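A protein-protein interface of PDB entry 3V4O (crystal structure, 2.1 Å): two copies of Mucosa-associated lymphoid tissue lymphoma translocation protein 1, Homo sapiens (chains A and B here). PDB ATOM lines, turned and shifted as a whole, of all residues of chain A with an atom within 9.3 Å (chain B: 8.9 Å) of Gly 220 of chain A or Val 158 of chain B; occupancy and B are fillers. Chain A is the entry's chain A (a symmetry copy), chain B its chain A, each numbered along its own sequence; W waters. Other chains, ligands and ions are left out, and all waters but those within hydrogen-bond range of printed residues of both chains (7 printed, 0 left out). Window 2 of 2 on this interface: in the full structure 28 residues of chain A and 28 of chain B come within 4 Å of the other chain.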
ATOM      1  N   LYS A 142     -22.706  -0.907  11.133  1.00  0.00           N
ATOM      2  CA  LYS A 142     -23.059  -0.151  12.336  1.00  0.00           C
ATOM      3  C   LYS A 142     -21.900  -0.184  13.287  1.00  0.00           C
ATOM      4  O   LYS A 142     -20.999  -1.016  13.138  1.00  0.00           O
ATOM      5  CB  LYS A 142     -24.295  -0.749  12.982  1.00  0.00           C
ATOM      6  CG  LYS A 142     -25.551  -0.533  12.134  1.00  0.00           C
ATOM      7  CD  LYS A 142     -26.780  -1.011  12.863  1.00  0.00           C
ATOM      8  CE  LYS A 142     -26.630  -2.471  13.223  1.00  0.00           C
ATOM      9  NZ  LYS A 142     -27.945  -3.036  13.674  1.00  0.00           N
ATOM     10  N   ALA A 167     -22.139  -3.285   0.298  1.00  0.00           N
ATOM     11  CA  ALA A 167     -23.551  -3.656   0.165  1.00  0.00           C
ATOM     12  C   ALA A 167     -24.446  -2.578   0.753  1.00  0.00           C
ATOM     13  O   ALA A 167     -25.581  -2.408   0.321  1.00  0.00           O
ATOM     14  CB  ALA A 167     -23.811  -4.970   0.893  1.00  0.00           C
ATOM     15  N   THR A 168     -23.946  -1.870   1.756  1.00  0.00           N
ATOM     16  CA  THR A 168     -24.764  -0.848   2.423  1.00  0.00           C
ATOM     17  C   THR A 168     -23.952   0.402   2.822  1.00  0.00           C
ATOM     18  O   THR A 168     -22.761   0.418   2.626  1.00  0.00           O
ATOM     19  CB  THR A 168     -25.535  -1.420   3.638  1.00  0.00           C
ATOM     20  OG1 THR A 168     -26.671  -0.577   3.889  1.00  0.00           O
ATOM     21  CG2 THR A 168     -24.650  -1.501   4.943  1.00  0.00           C
ATOM     22  N   CYS A 169     -24.614   1.443   3.343  1.00  0.00           N
ATOM     23  CA  CYS A 169     -23.973   2.672   3.768  1.00  0.00           C
ATOM     24  C   CYS A 169     -23.508   2.604   5.234  1.00  0.00           C
ATOM     25  O   CYS A 169     -23.975   1.761   6.022  1.00  0.00           O
ATOM     26  CB  CYS A 169     -24.953   3.864   3.622  1.00  0.00           C
ATOM     27  SG  CYS A 169     -25.389   4.188   1.900  1.00  0.00           S
ATOM     28  N   GLN A 170     -22.565   3.480   5.583  1.00  0.00           N
ATOM     29  CA  GLN A 170     -22.028   3.522   6.945  1.00  0.00           C
ATOM     30  C   GLN A 170     -23.146   3.748   7.945  1.00  0.00           C
ATOM     31  O   GLN A 170     -24.028   4.570   7.694  1.00  0.00           O
ATOM     32  CB  GLN A 170     -21.030   4.653   7.051  1.00  0.00           C
ATOM     33  CG  GLN A 170     -20.241   4.712   8.356  1.00  0.00           C
ATOM     34  CD  GLN A 170     -19.071   5.690   8.226  1.00  0.00           C
ATOM     35  OE1 GLN A 170     -19.281   6.887   8.047  1.00  0.00           O
ATOM     36  NE2 GLN A 170     -17.835   5.175   8.292  1.00  0.00           N
ATOM     37  N   GLY A 171     -23.104   3.023   9.070  1.00  0.00           N
ATOM     38  CA  GLY A 171     -24.147   3.125  10.101  1.00  0.00           C
ATOM     39  C   GLY A 171     -25.430   2.405   9.708  1.00  0.00           C
ATOM     40  O   GLY A 171     -26.450   2.519  10.381  1.00  0.00           O
ATOM     41  N   ALA A 172     -25.403   1.664   8.606  1.00  0.00           N
ATOM     42  CA  ALA A 172     -26.621   0.987   8.166  1.00  0.00           C
ATOM     43  C   ALA A 172     -26.434  -0.546   8.057  1.00  0.00           C
ATOM     44  O   ALA A 172     -25.320  -1.076   8.225  1.00  0.00           O
ATOM     45  CB  ALA A 172     -27.054   1.553   6.854  1.00  0.00           C
ATOM     46  N   GLU A 173     -27.515  -1.251   7.742  1.00  0.00           N
ATOM     47  CA  GLU A 173     -27.476  -2.709   7.698  1.00  0.00           C
ATOM     48  C   GLU A 173     -27.493  -3.186   6.258  1.00  0.00           C
ATOM     49  O   GLU A 173     -27.986  -2.483   5.385  1.00  0.00           O
ATOM     50  CB  GLU A 173     -28.678  -3.280   8.492  1.00  0.00           C
ATOM     51  CG  GLU A 173     -28.537  -3.102  10.000  1.00  0.00           C
ATOM     52  CD  GLU A 173     -29.750  -3.671  10.808  1.00  0.00           C
ATOM     53  OE1 GLU A 173     -30.904  -3.393  10.469  1.00  0.00           O
ATOM     54  OE2 GLU A 173     -29.542  -4.399  11.786  1.00  0.00           O
ATOM     55  N   ALA A 174     -26.928  -4.372   6.011  1.00  0.00           N
ATOM     56  CA  ALA A 174     -27.048  -5.046   4.742  1.00  0.00           C
ATOM     57  C   ALA A 174     -27.905  -6.300   5.002  1.00  0.00           C
ATOM     58  O   ALA A 174     -27.854  -6.864   6.097  1.00  0.00           O
ATOM     59  CB  ALA A 174     -25.675  -5.449   4.235  1.00  0.00           C
ATOM     60  N   PHE A 175     -28.652  -6.745   4.004  1.00  0.00           N
ATOM     61  CA  PHE A 175     -29.702  -7.745   4.222  1.00  0.00           C
ATOM     62  C   PHE A 175     -29.664  -8.961   3.301  1.00  0.00           C
ATOM     63  O   PHE A 175     -29.071  -8.956   2.219  1.00  0.00           O
ATOM     64  CB  PHE A 175     -31.099  -7.099   4.117  1.00  0.00           C
ATOM     65  CG  PHE A 175     -31.354  -6.027   5.154  1.00  0.00           C
ATOM     66  CD1 PHE A 175     -31.744  -6.364   6.448  1.00  0.00           C
ATOM     67  CD2 PHE A 175     -31.226  -4.690   4.830  1.00  0.00           C
ATOM     68  CE1 PHE A 175     -31.981  -5.374   7.409  1.00  0.00           C
ATOM     69  CE2 PHE A 175     -31.469  -3.692   5.787  1.00  0.00           C
ATOM     70  CZ  PHE A 175     -31.859  -4.046   7.069  1.00  0.00           C
ATOM     71  N   MET A 212     -30.466  -1.815  -7.488  1.00  0.00           N
ATOM     72  CA  MET A 212     -30.840  -2.071  -6.104  1.00  0.00           C
ATOM     73  C   MET A 212     -31.826  -1.024  -5.612  1.00  0.00           C
ATOM     74  O   MET A 212     -32.700  -1.304  -4.753  1.00  0.00           O
ATOM     75  CB  MET A 212     -29.616  -2.115  -5.199  1.00  0.00           C
ATOM     76  CG  MET A 212     -29.942  -2.433  -3.731  1.00  0.00           C
ATOM     77  SD  MET A 212     -28.521  -2.411  -2.580  1.00  0.00           S
ATOM     78  CE  MET A 212     -27.351  -3.399  -3.523  1.00  0.00           C
ATOM     79  N   GLY A 213     -31.715   0.185  -6.156  1.00  0.00           N
ATOM     80  CA  GLY A 213     -32.637   1.241  -5.725  1.00  0.00           C
ATOM     81  C   GLY A 213     -34.084   0.988  -6.134  1.00  0.00           C
ATOM     82  O   GLY A 213     -34.979   1.658  -5.653  1.00  0.00           O
ATOM     83  N   CYS A 215     -35.521  -1.939  -5.603  1.00  0.00           N
ATOM     84  CA  CYS A 215     -35.956  -3.023  -4.748  1.00  0.00           C
ATOM     85  C   CYS A 215     -36.726  -2.459  -3.572  1.00  0.00           C
ATOM     86  O   CYS A 215     -36.188  -1.741  -2.727  1.00  0.00           O
ATOM     87  CB  CYS A 215     -34.761  -3.834  -4.264  1.00  0.00           C
ATOM     88  SG  CYS A 215     -35.180  -5.074  -3.047  1.00  0.00           S
ATOM     89  N   HIS A 216     -38.007  -2.796  -3.536  1.00  0.00           N
ATOM     90  CA  HIS A 216     -38.923  -2.289  -2.547  1.00  0.00           C
ATOM     91  C   HIS A 216     -38.576  -2.705  -1.141  1.00  0.00           C
ATOM     92  O   HIS A 216     -38.667  -1.909  -0.241  1.00  0.00           O
ATOM     93  CB  HIS A 216     -40.352  -2.726  -2.917  1.00  0.00           C
ATOM     94  CG  HIS A 216     -40.916  -1.963  -4.075  1.00  0.00           C
ATOM     95  ND1 HIS A 216     -41.035  -2.505  -5.340  1.00  0.00           N
ATOM     96  CD2 HIS A 216     -41.348  -0.680  -4.168  1.00  0.00           C
ATOM     97  CE1 HIS A 216     -41.541  -1.595  -6.160  1.00  0.00           C
ATOM     98  NE2 HIS A 216     -41.738  -0.480  -5.475  1.00  0.00           N
ATOM     99  N   LEU A 217     -38.152  -3.949  -0.958  1.00  0.00           N
ATOM    100  CA  LEU A 217     -37.799  -4.452   0.365  1.00  0.00           C
ATOM    101  C   LEU A 217     -36.788  -3.579   1.102  1.00  0.00           C
ATOM    102  O   LEU A 217     -36.854  -3.434   2.318  1.00  0.00           O
ATOM    103  CB  LEU A 217     -37.225  -5.873   0.266  1.00  0.00           C
ATOM    104  CG  LEU A 217     -37.947  -7.087   0.804  1.00  0.00           C
ATOM    105  CD1 LEU A 217     -36.939  -8.223   0.984  1.00  0.00           C
ATOM    106  CD2 LEU A 217     -38.730  -6.782   2.099  1.00  0.00           C
ATOM    107  N   THR A 218     -35.844  -2.995   0.381  1.00  0.00           N
ATOM    108  CA  THR A 218     -34.734  -2.318   1.060  1.00  0.00           C
ATOM    109  C   THR A 218     -34.756  -0.773   1.014  1.00  0.00           C
ATOM    110  O   THR A 218     -33.876  -0.113   1.589  1.00  0.00           O
ATOM    111  CB  THR A 218     -33.390  -2.861   0.539  1.00  0.00           C
ATOM    112  OG1 THR A 218     -33.368  -2.759  -0.893  1.00  0.00           O
ATOM    113  CG2 THR A 218     -33.239  -4.333   0.954  1.00  0.00           C
ATOM    114  N   LYS A 219     -35.770  -0.195   0.366  1.00  0.00           N
ATOM    115  CA  LYS A 219     -35.870   1.270   0.311  1.00  0.00           C
ATOM    116  C   LYS A 219     -35.772   1.846   1.695  1.00  0.00           C
ATOM    117  O   LYS A 219     -36.459   1.402   2.600  1.00  0.00           O
ATOM    118  CB  LYS A 219     -37.170   1.734  -0.369  1.00  0.00           C
ATOM    119  CG  LYS A 219     -37.265   1.223  -1.804  1.00  0.00           C
ATOM    120  CD  LYS A 219     -37.788   2.264  -2.820  1.00  0.00           C
ATOM    121  CE  LYS A 219     -38.081   1.568  -4.164  1.00  0.00           C
ATOM    122  NZ  LYS A 219     -38.293   2.504  -5.316  1.00  0.00           N
ATOM    123  N   GLY A 220     -34.884   2.809   1.878  1.00  0.00           N
ATOM    124  CA  GLY A 220     -34.730   3.454   3.166  1.00  0.00           C
ATOM    125  C   GLY A 220     -33.911   2.682   4.187  1.00  0.00           C
ATOM    126  O   GLY A 220     -33.777   3.116   5.343  1.00  0.00           O
ATOM    127  N   LYS A 221     -33.365   1.528   3.814  1.00  0.00           N
ATOM    128  CA  LYS A 221     -32.558   0.808   4.807  1.00  0.00           C
ATOM    129  C   LYS A 221     -31.246   0.206   4.303  1.00  0.00           C
ATOM    130  O   LYS A 221     -30.321   0.028   5.088  1.00  0.00           O
ATOM    131  CB  LYS A 221     -33.363  -0.243   5.573  1.00  0.00           C
ATOM    132  CG  LYS A 221     -34.373  -1.018   4.795  1.00  0.00           C
ATOM    133  CD  LYS A 221     -35.151  -1.888   5.785  1.00  0.00           C
ATOM    134  CE  LYS A 221     -36.602  -2.003   5.418  1.00  0.00           C
ATOM    135  NZ  LYS A 221     -37.372  -2.309   6.652  1.00  0.00           N
ATOM    136  N   GLN A 222     -31.184  -0.117   3.018  1.00  0.00           N
ATOM    137  CA  GLN A 222     -29.924  -0.546   2.424  1.00  0.00           C
ATOM    138  C   GLN A 222     -29.724   0.127   1.061  1.00  0.00           C
ATOM    139  O   GLN A 222     -30.605   0.110   0.207  1.00  0.00           O
ATOM    140  CB  GLN A 222     -29.853  -2.065   2.269  1.00  0.00           C
ATOM    141  CG  GLN A 222     -28.725  -2.544   1.332  1.00  0.00           C
ATOM    142  CD  GLN A 222     -28.520  -4.049   1.403  1.00  0.00           C
ATOM    143  OE1 GLN A 222     -29.312  -4.766   2.034  1.00  0.00           O
ATOM    144  NE2 GLN A 222     -27.469  -4.536   0.757  1.00  0.00           N
ATOM    145  N   ALA A 223     -28.532   0.678   0.856  1.00  0.00           N
ATOM    146  CA  ALA A 223     -28.156   1.187  -0.461  1.00  0.00           C
ATOM    147  C   ALA A 223     -26.674   0.938  -0.701  1.00  0.00           C
ATOM    148  O   ALA A 223     -25.852   1.164   0.189  1.00  0.00           O
ATOM    149  CB  ALA A 223     -28.475   2.687  -0.552  1.00  0.00           C
ATOM    150  N   LEU A 224     -26.351   0.465  -1.904  1.00  0.00           N
ATOM    151  CA  LEU A 224     -25.000   0.225  -2.269  1.00  0.00           C
ATOM    152  C   LEU A 224     -24.197   1.528  -2.094  1.00  0.00           C
ATOM    153  O   LEU A 224     -24.676   2.595  -2.465  1.00  0.00           O
ATOM    154  CB  LEU A 224     -24.968  -0.204  -3.734  1.00  0.00           C
ATOM    155  CG  LEU A 224     -23.807  -1.105  -4.168  1.00  0.00           C
ATOM    156  CD1 LEU A 224     -24.153  -1.789  -5.458  1.00  0.00           C
ATOM    157  CD2 LEU A 224     -22.550  -0.308  -4.377  1.00  0.00           C
ATOM    158  N   GLU A 225     -23.008   1.438  -1.496  1.00  0.00           N
ATOM    159  CA  GLU A 225     -22.060   2.547  -1.503  1.00  0.00           C
ATOM    160  C   GLU A 225     -20.784   2.192  -2.270  1.00  0.00           C
ATOM    161  O   GLU A 225     -20.120   1.188  -2.003  1.00  0.00           O
ATOM    162  CB  GLU A 225     -21.722   3.061  -0.087  1.00  0.00           C
ATOM    163  CG  GLU A 225     -20.913   4.366  -0.155  1.00  0.00           C
ATOM    164  CD  GLU A 225     -20.697   5.029   1.182  1.00  0.00           C
ATOM    165  OE1 GLU A 225     -20.014   4.426   2.042  1.00  0.00           O
ATOM    166  OE2 GLU A 225     -21.212   6.165   1.364  1.00  0.00           O
ATOM    167  N   GLN B 126     -30.217  16.344   4.728  1.00  0.00           N
ATOM    168  CA  GLN B 126     -31.136  15.231   4.600  1.00  0.00           C
ATOM    169  C   GLN B 126     -32.437  15.548   5.312  1.00  0.00           C
ATOM    170  O   GLN B 126     -33.479  15.136   4.855  1.00  0.00           O
ATOM    171  CB  GLN B 126     -30.571  13.941   5.180  1.00  0.00           C
ATOM    172  CG  GLN B 126     -29.422  13.368   4.417  1.00  0.00           C
ATOM    173  CD  GLN B 126     -28.962  12.069   5.042  1.00  0.00           C
ATOM    174  OE1 GLN B 126     -29.043  10.990   4.434  1.00  0.00           O
ATOM    175  NE2 GLN B 126     -28.493  12.163   6.274  1.00  0.00           N
ATOM    176  N   ASN B 133     -27.627  15.285  -2.890  1.00  0.00           N
ATOM    177  CA  ASN B 133     -26.600  15.948  -2.061  1.00  0.00           C
ATOM    178  C   ASN B 133     -25.204  15.712  -2.622  1.00  0.00           C
ATOM    179  O   ASN B 133     -24.729  14.569  -2.623  1.00  0.00           O
ATOM    180  CB  ASN B 133     -26.609  15.424  -0.615  1.00  0.00           C
ATOM    181  CG  ASN B 133     -28.023  15.410   0.012  1.00  0.00           C
ATOM    182  OD1 ASN B 133     -28.629  16.459   0.223  1.00  0.00           O
ATOM    183  ND2 ASN B 133     -28.534  14.204   0.325  1.00  0.00           N
ATOM    184  N   ALA B 155     -25.939   7.763  13.072  1.00  0.00           N
ATOM    185  CA  ALA B 155     -25.943   7.243  11.717  1.00  0.00           C
ATOM    186  C   ALA B 155     -26.865   8.105  10.835  1.00  0.00           C
ATOM    187  O   ALA B 155     -27.902   8.593  11.291  1.00  0.00           O
ATOM    188  CB  ALA B 155     -26.373   5.783  11.698  1.00  0.00           C
ATOM    189  N   LEU B 156     -26.473   8.310   9.581  1.00  0.00           N
ATOM    190  CA  LEU B 156     -27.329   9.038   8.669  1.00  0.00           C
ATOM    191  C   LEU B 156     -28.406   8.130   8.104  1.00  0.00           C
ATOM    192  O   LEU B 156     -28.190   6.920   7.979  1.00  0.00           O
ATOM    193  CB  LEU B 156     -26.487   9.623   7.528  1.00  0.00           C
ATOM    194  CG  LEU B 156     -25.273  10.492   7.880  1.00  0.00           C
ATOM    195  CD1 LEU B 156     -24.463  10.734   6.611  1.00  0.00           C
ATOM    196  CD2 LEU B 156     -25.666  11.810   8.511  1.00  0.00           C
ATOM    197  N   LYS B 157     -29.553   8.702   7.742  1.00  0.00           N
ATOM    198  CA  LYS B 157     -30.556   7.969   6.978  1.00  0.00           C
ATOM    199  C   LYS B 157     -29.986   7.461   5.680  1.00  0.00           C
ATOM    200  O   LYS B 157     -29.081   8.077   5.088  1.00  0.00           O
ATOM    201  CB  LYS B 157     -31.751   8.842   6.603  1.00  0.00           C
ATOM    202  CG  LYS B 157     -32.484   9.482   7.765  1.00  0.00           C
ATOM    203  CD  LYS B 157     -33.823  10.043   7.262  1.00  0.00           C
ATOM    204  CE  LYS B 157     -34.003  11.516   7.645  1.00  0.00           C
ATOM    205  NZ  LYS B 157     -33.780  11.744   9.106  1.00  0.00           N
ATOM    206  N   VAL B 158     -30.568   6.368   5.200  1.00  0.00           N
ATOM    207  CA  VAL B 158     -30.249   5.835   3.891  1.00  0.00           C
ATOM    208  C   VAL B 158     -31.119   6.520   2.839  1.00  0.00           C
ATOM    209  O   VAL B 158     -32.259   6.094   2.564  1.00  0.00           O
ATOM    210  CB  VAL B 158     -30.448   4.307   3.853  1.00  0.00           C
ATOM    211  CG1 VAL B 158     -30.052   3.750   2.494  1.00  0.00           C
ATOM    212  CG2 VAL B 158     -29.612   3.668   4.952  1.00  0.00           C
ATOM    213  N   THR B 159     -30.598   7.595   2.249  1.00  0.00           N
ATOM    214  CA  THR B 159     -31.414   8.366   1.272  1.00  0.00           C
ATOM    215  C   THR B 159     -30.991   8.020  -0.151  1.00  0.00           C
ATOM    216  O   THR B 159     -31.616   8.434  -1.119  1.00  0.00           O
ATOM    217  CB  THR B 159     -31.333   9.892   1.539  1.00  0.00           C
ATOM    218  OG1 THR B 159     -29.955  10.292   1.753  1.00  0.00           O
ATOM    219  CG2 THR B 159     -32.136  10.240   2.790  1.00  0.00           C
ATOM    220  N   ALA B 160     -29.883   7.291  -0.272  1.00  0.00           N
ATOM    221  CA  ALA B 160     -29.437   6.812  -1.562  1.00  0.00           C
ATOM    222  C   ALA B 160     -29.260   7.949  -2.583  1.00  0.00           C
ATOM    223  O   ALA B 160     -29.587   7.778  -3.752  1.00  0.00           O
ATOM    224  CB  ALA B 160     -30.456   5.740  -2.088  1.00  0.00           C
ATOM    225  N   ASN B 161     -28.746   9.103  -2.152  1.00  0.00           N
ATOM    226  CA  ASN B 161     -28.683  10.263  -3.050  1.00  0.00           C
ATOM    227  C   ASN B 161     -27.521  11.194  -2.712  1.00  0.00           C
ATOM    228  O   ASN B 161     -27.624  12.410  -2.839  1.00  0.00           O
ATOM    229  CB  ASN B 161     -30.017  11.032  -2.966  1.00  0.00           C
ATOM    230  CG  ASN B 161     -30.276  11.550  -1.587  1.00  0.00           C
ATOM    231  OD1 ASN B 161     -29.522  11.245  -0.651  1.00  0.00           O
ATOM    232  ND2 ASN B 161     -31.314  12.392  -1.438  1.00  0.00           N
ATOM    233  N   ILE B 162     -26.428  10.597  -2.257  1.00  0.00           N
ATOM    234  CA  ILE B 162     -25.299  11.317  -1.719  1.00  0.00           C
ATOM    235  C   ILE B 162     -24.084  11.026  -2.578  1.00  0.00           C
ATOM    236  O   ILE B 162     -23.744   9.850  -2.796  1.00  0.00           O
ATOM    237  CB  ILE B 162     -25.010  10.833  -0.286  1.00  0.00           C
ATOM    238  CG1 ILE B 162     -26.235  11.120   0.592  1.00  0.00           C
ATOM    239  CG2 ILE B 162     -23.709  11.475   0.256  1.00  0.00           C
ATOM    240  CD1 ILE B 162     -26.269  10.365   1.904  1.00  0.00           C
ATOM    241  N   SER B 229     -23.634   6.935  -2.810  1.00  0.00           N
ATOM    242  CA  SER B 229     -24.741   5.995  -2.677  1.00  0.00           C
ATOM    243  C   SER B 229     -25.917   6.421  -3.563  1.00  0.00           C
ATOM    244  O   SER B 229     -27.043   5.952  -3.407  1.00  0.00           O
ATOM    245  CB  SER B 229     -25.151   5.854  -1.204  1.00  0.00           C
ATOM    246  OG  SER B 229     -25.620   7.073  -0.658  1.00  0.00           O
ATOM    247  N   SER B 231     -28.458   6.156  -6.112  1.00  0.00           N
ATOM    248  CA  SER B 231     -28.975   5.084  -6.950  1.00  0.00           C
ATOM    249  C   SER B 231     -29.614   5.651  -8.223  1.00  0.00           C
ATOM    250  O   SER B 231     -29.253   5.247  -9.328  1.00  0.00           O
ATOM    251  CB  SER B 231     -29.941   4.122  -6.204  1.00  0.00           C
ATOM    252  OG  SER B 231     -30.748   4.808  -5.273  1.00  0.00           O
HETATM  253  O   HOH W   1     -26.417   5.267   6.299  1.00  0.00           O
HETATM  254  O   HOH W   2     -23.285   7.829   0.833  1.00  0.00           O
HETATM  255  O   HOH W   3     -24.015   7.213   8.832  1.00  0.00           O
HETATM  256  O   HOH W   4     -26.746   6.897   4.114  1.00  0.00           O
HETATM  257  O   HOH W   5     -32.481   5.175   6.722  1.00  0.00           O
HETATM  258  O   HOH W   6     -26.905   3.239  -3.781  1.00  0.00           O
HETATM  259  O   HOH W   7     -27.544   6.842   1.283  1.00  0.00           O
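O of Ala 160 of chain B lies within hydrogen-bond range of N of Ser 231 of chain B, 3.1 Å away.
The backbone carbonyl oxygen of Ala 167 of chain A sits at hydrogen-bond distance from the side-chain amide nitrogen of Gln 222 of chain A, at 2.9 Å.
The backbone NH (N) of Cys 169 of chain A is in hydrogen-bond range of the backbone carbonyl oxygen (O) of Ala 223 of chain A (3.4 Å).
N of Phe 175 of chain A is in hydrogen-bond range of OE1 of Gln 222 of chain A (2.9 Å).
The backbone NH of Leu 224 of chain A sits at hydrogen-bond distance from the side-chain sulfur of Met 212 of chain A, at 3.7 Å.
The side-chain amino group (NZ) of Lys 219 of chain A is in hydrogen-bond range of the backbone carbonyl oxygen (O) of Gly 213 of chain A, at 3.4 Å.
Ser 229 of chain B touches Cys 169 of chain A (CB to SG, 3.5 Å).
Ala 155 of chain B touches Gly 171 of chain A (CB to O, 3.5 Å).
Ala 172 of chain A touches Val 158 of chain B.
Gly 213 of chain A touches Ser 231 of chain B.
O of Val 158 of chain B touches CA of Gly 220 of chain A, 3.7 Å away.
Lys 221 of chain A touches Val 158 of chain B (O to CG2, 3.7 Å).
CG1 of Val 158 of chain B touches C of Gln 222 of chain A, 3.9 Å away.
Ala 223 of chain A touches Val 158 of chain B (CB to CG1, 3.6 Å).
CB of Ala 223 of chain A touches CB of Ala 160 of chain B, at 3.95 Å.
Leu 224 of chain A touches Ser 229 of chain B.
Of the printed residues of chain B, Lys 221 of chain A touches Val 158.
Of the printed residues of chain B, Ala 223 of chain A touches Val 158 and Ala 160.
Of the printed residues of chain A, Ala 155 of chain B touches Gly 171.
Of chain A, only Ala 172 (3.8 Å), Gly 220 (3.7 Å), Lys 221 (3.7 Å), Gln 222 (3.9 Å) and Ala 223 (3.6 Å) come within 4 Å of Val 158 of chain B.
No residue of chain A comes within 4 Å of Thr 159 of chain B.
The nearest residue of chain A that does not touch Val 158 of chain B is Cys 169 of chain A (4.7 Å).
Printed residues of chain A that touch a printed residue of chain B: Cys 169, Gly 171, Ala 172, Gly 213, Gly 220, Lys 221, Gln 222, Ala 223 and Leu 224.
Hydrophobic or aromatic side chains of chain A within 4 Å of the printed part of chain B: Ala 172 and Ala 223.
Hydrophobic or aromatic side chains of chain B that line the printed part of chain A: Ala 155, Val 158 and Ala 160.
Among the printed residues, 10 pairs touch across the chains.
Among the printed residues, no Asp or Glu carboxylate lies within 4 Å of a Lys or Arg side-chain nitrogen of the other chain.
No position is printed for both chains.
Of the 10 pairs that touch across the chains among the printed residues, none has its exchanged pair printed and touching as well.
Water W6 lies within hydrogen-bond range of the backbone carbonyl oxygen (O) of Leu 224 of chain A and the backbone carbonyl oxygen (O) of Ser 229 of chain B.
Water W2 lies within hydrogen-bond range of the side-chain carboxylate (OE2) of Glu 225 of chain A (2.7 Å) and the side-chain hydroxyl (OG) of Ser 229 of chain B (2.9 Å).
Water W7 lies within hydrogen-bond range of the side-chain hydroxyl of Ser 229 of chain B (2.7 Å), the backbone NH of Ala 160 of chain B (2.8 Å), the backbone NH of Thr 159 of chain B (3.3 Å) and the side-chain sulfur of Cys 169 of chain A (3.5 Å).
Water W4 bridges O of Lys 157 of chain B and SG of Cys 169 of chain A.
Water W3 lies within hydrogen-bond range of the backbone NH (N) of Leu 156 of chain B (2.8 Å) and the backbone carbonyl oxygen (O) of Gln 170 of chain A (2.9 Å).
Water W1 lies within hydrogen-bond range of O of Gln 170 of chain A (2.9 Å) and O of Leu 156 of chain B (2.9 Å).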
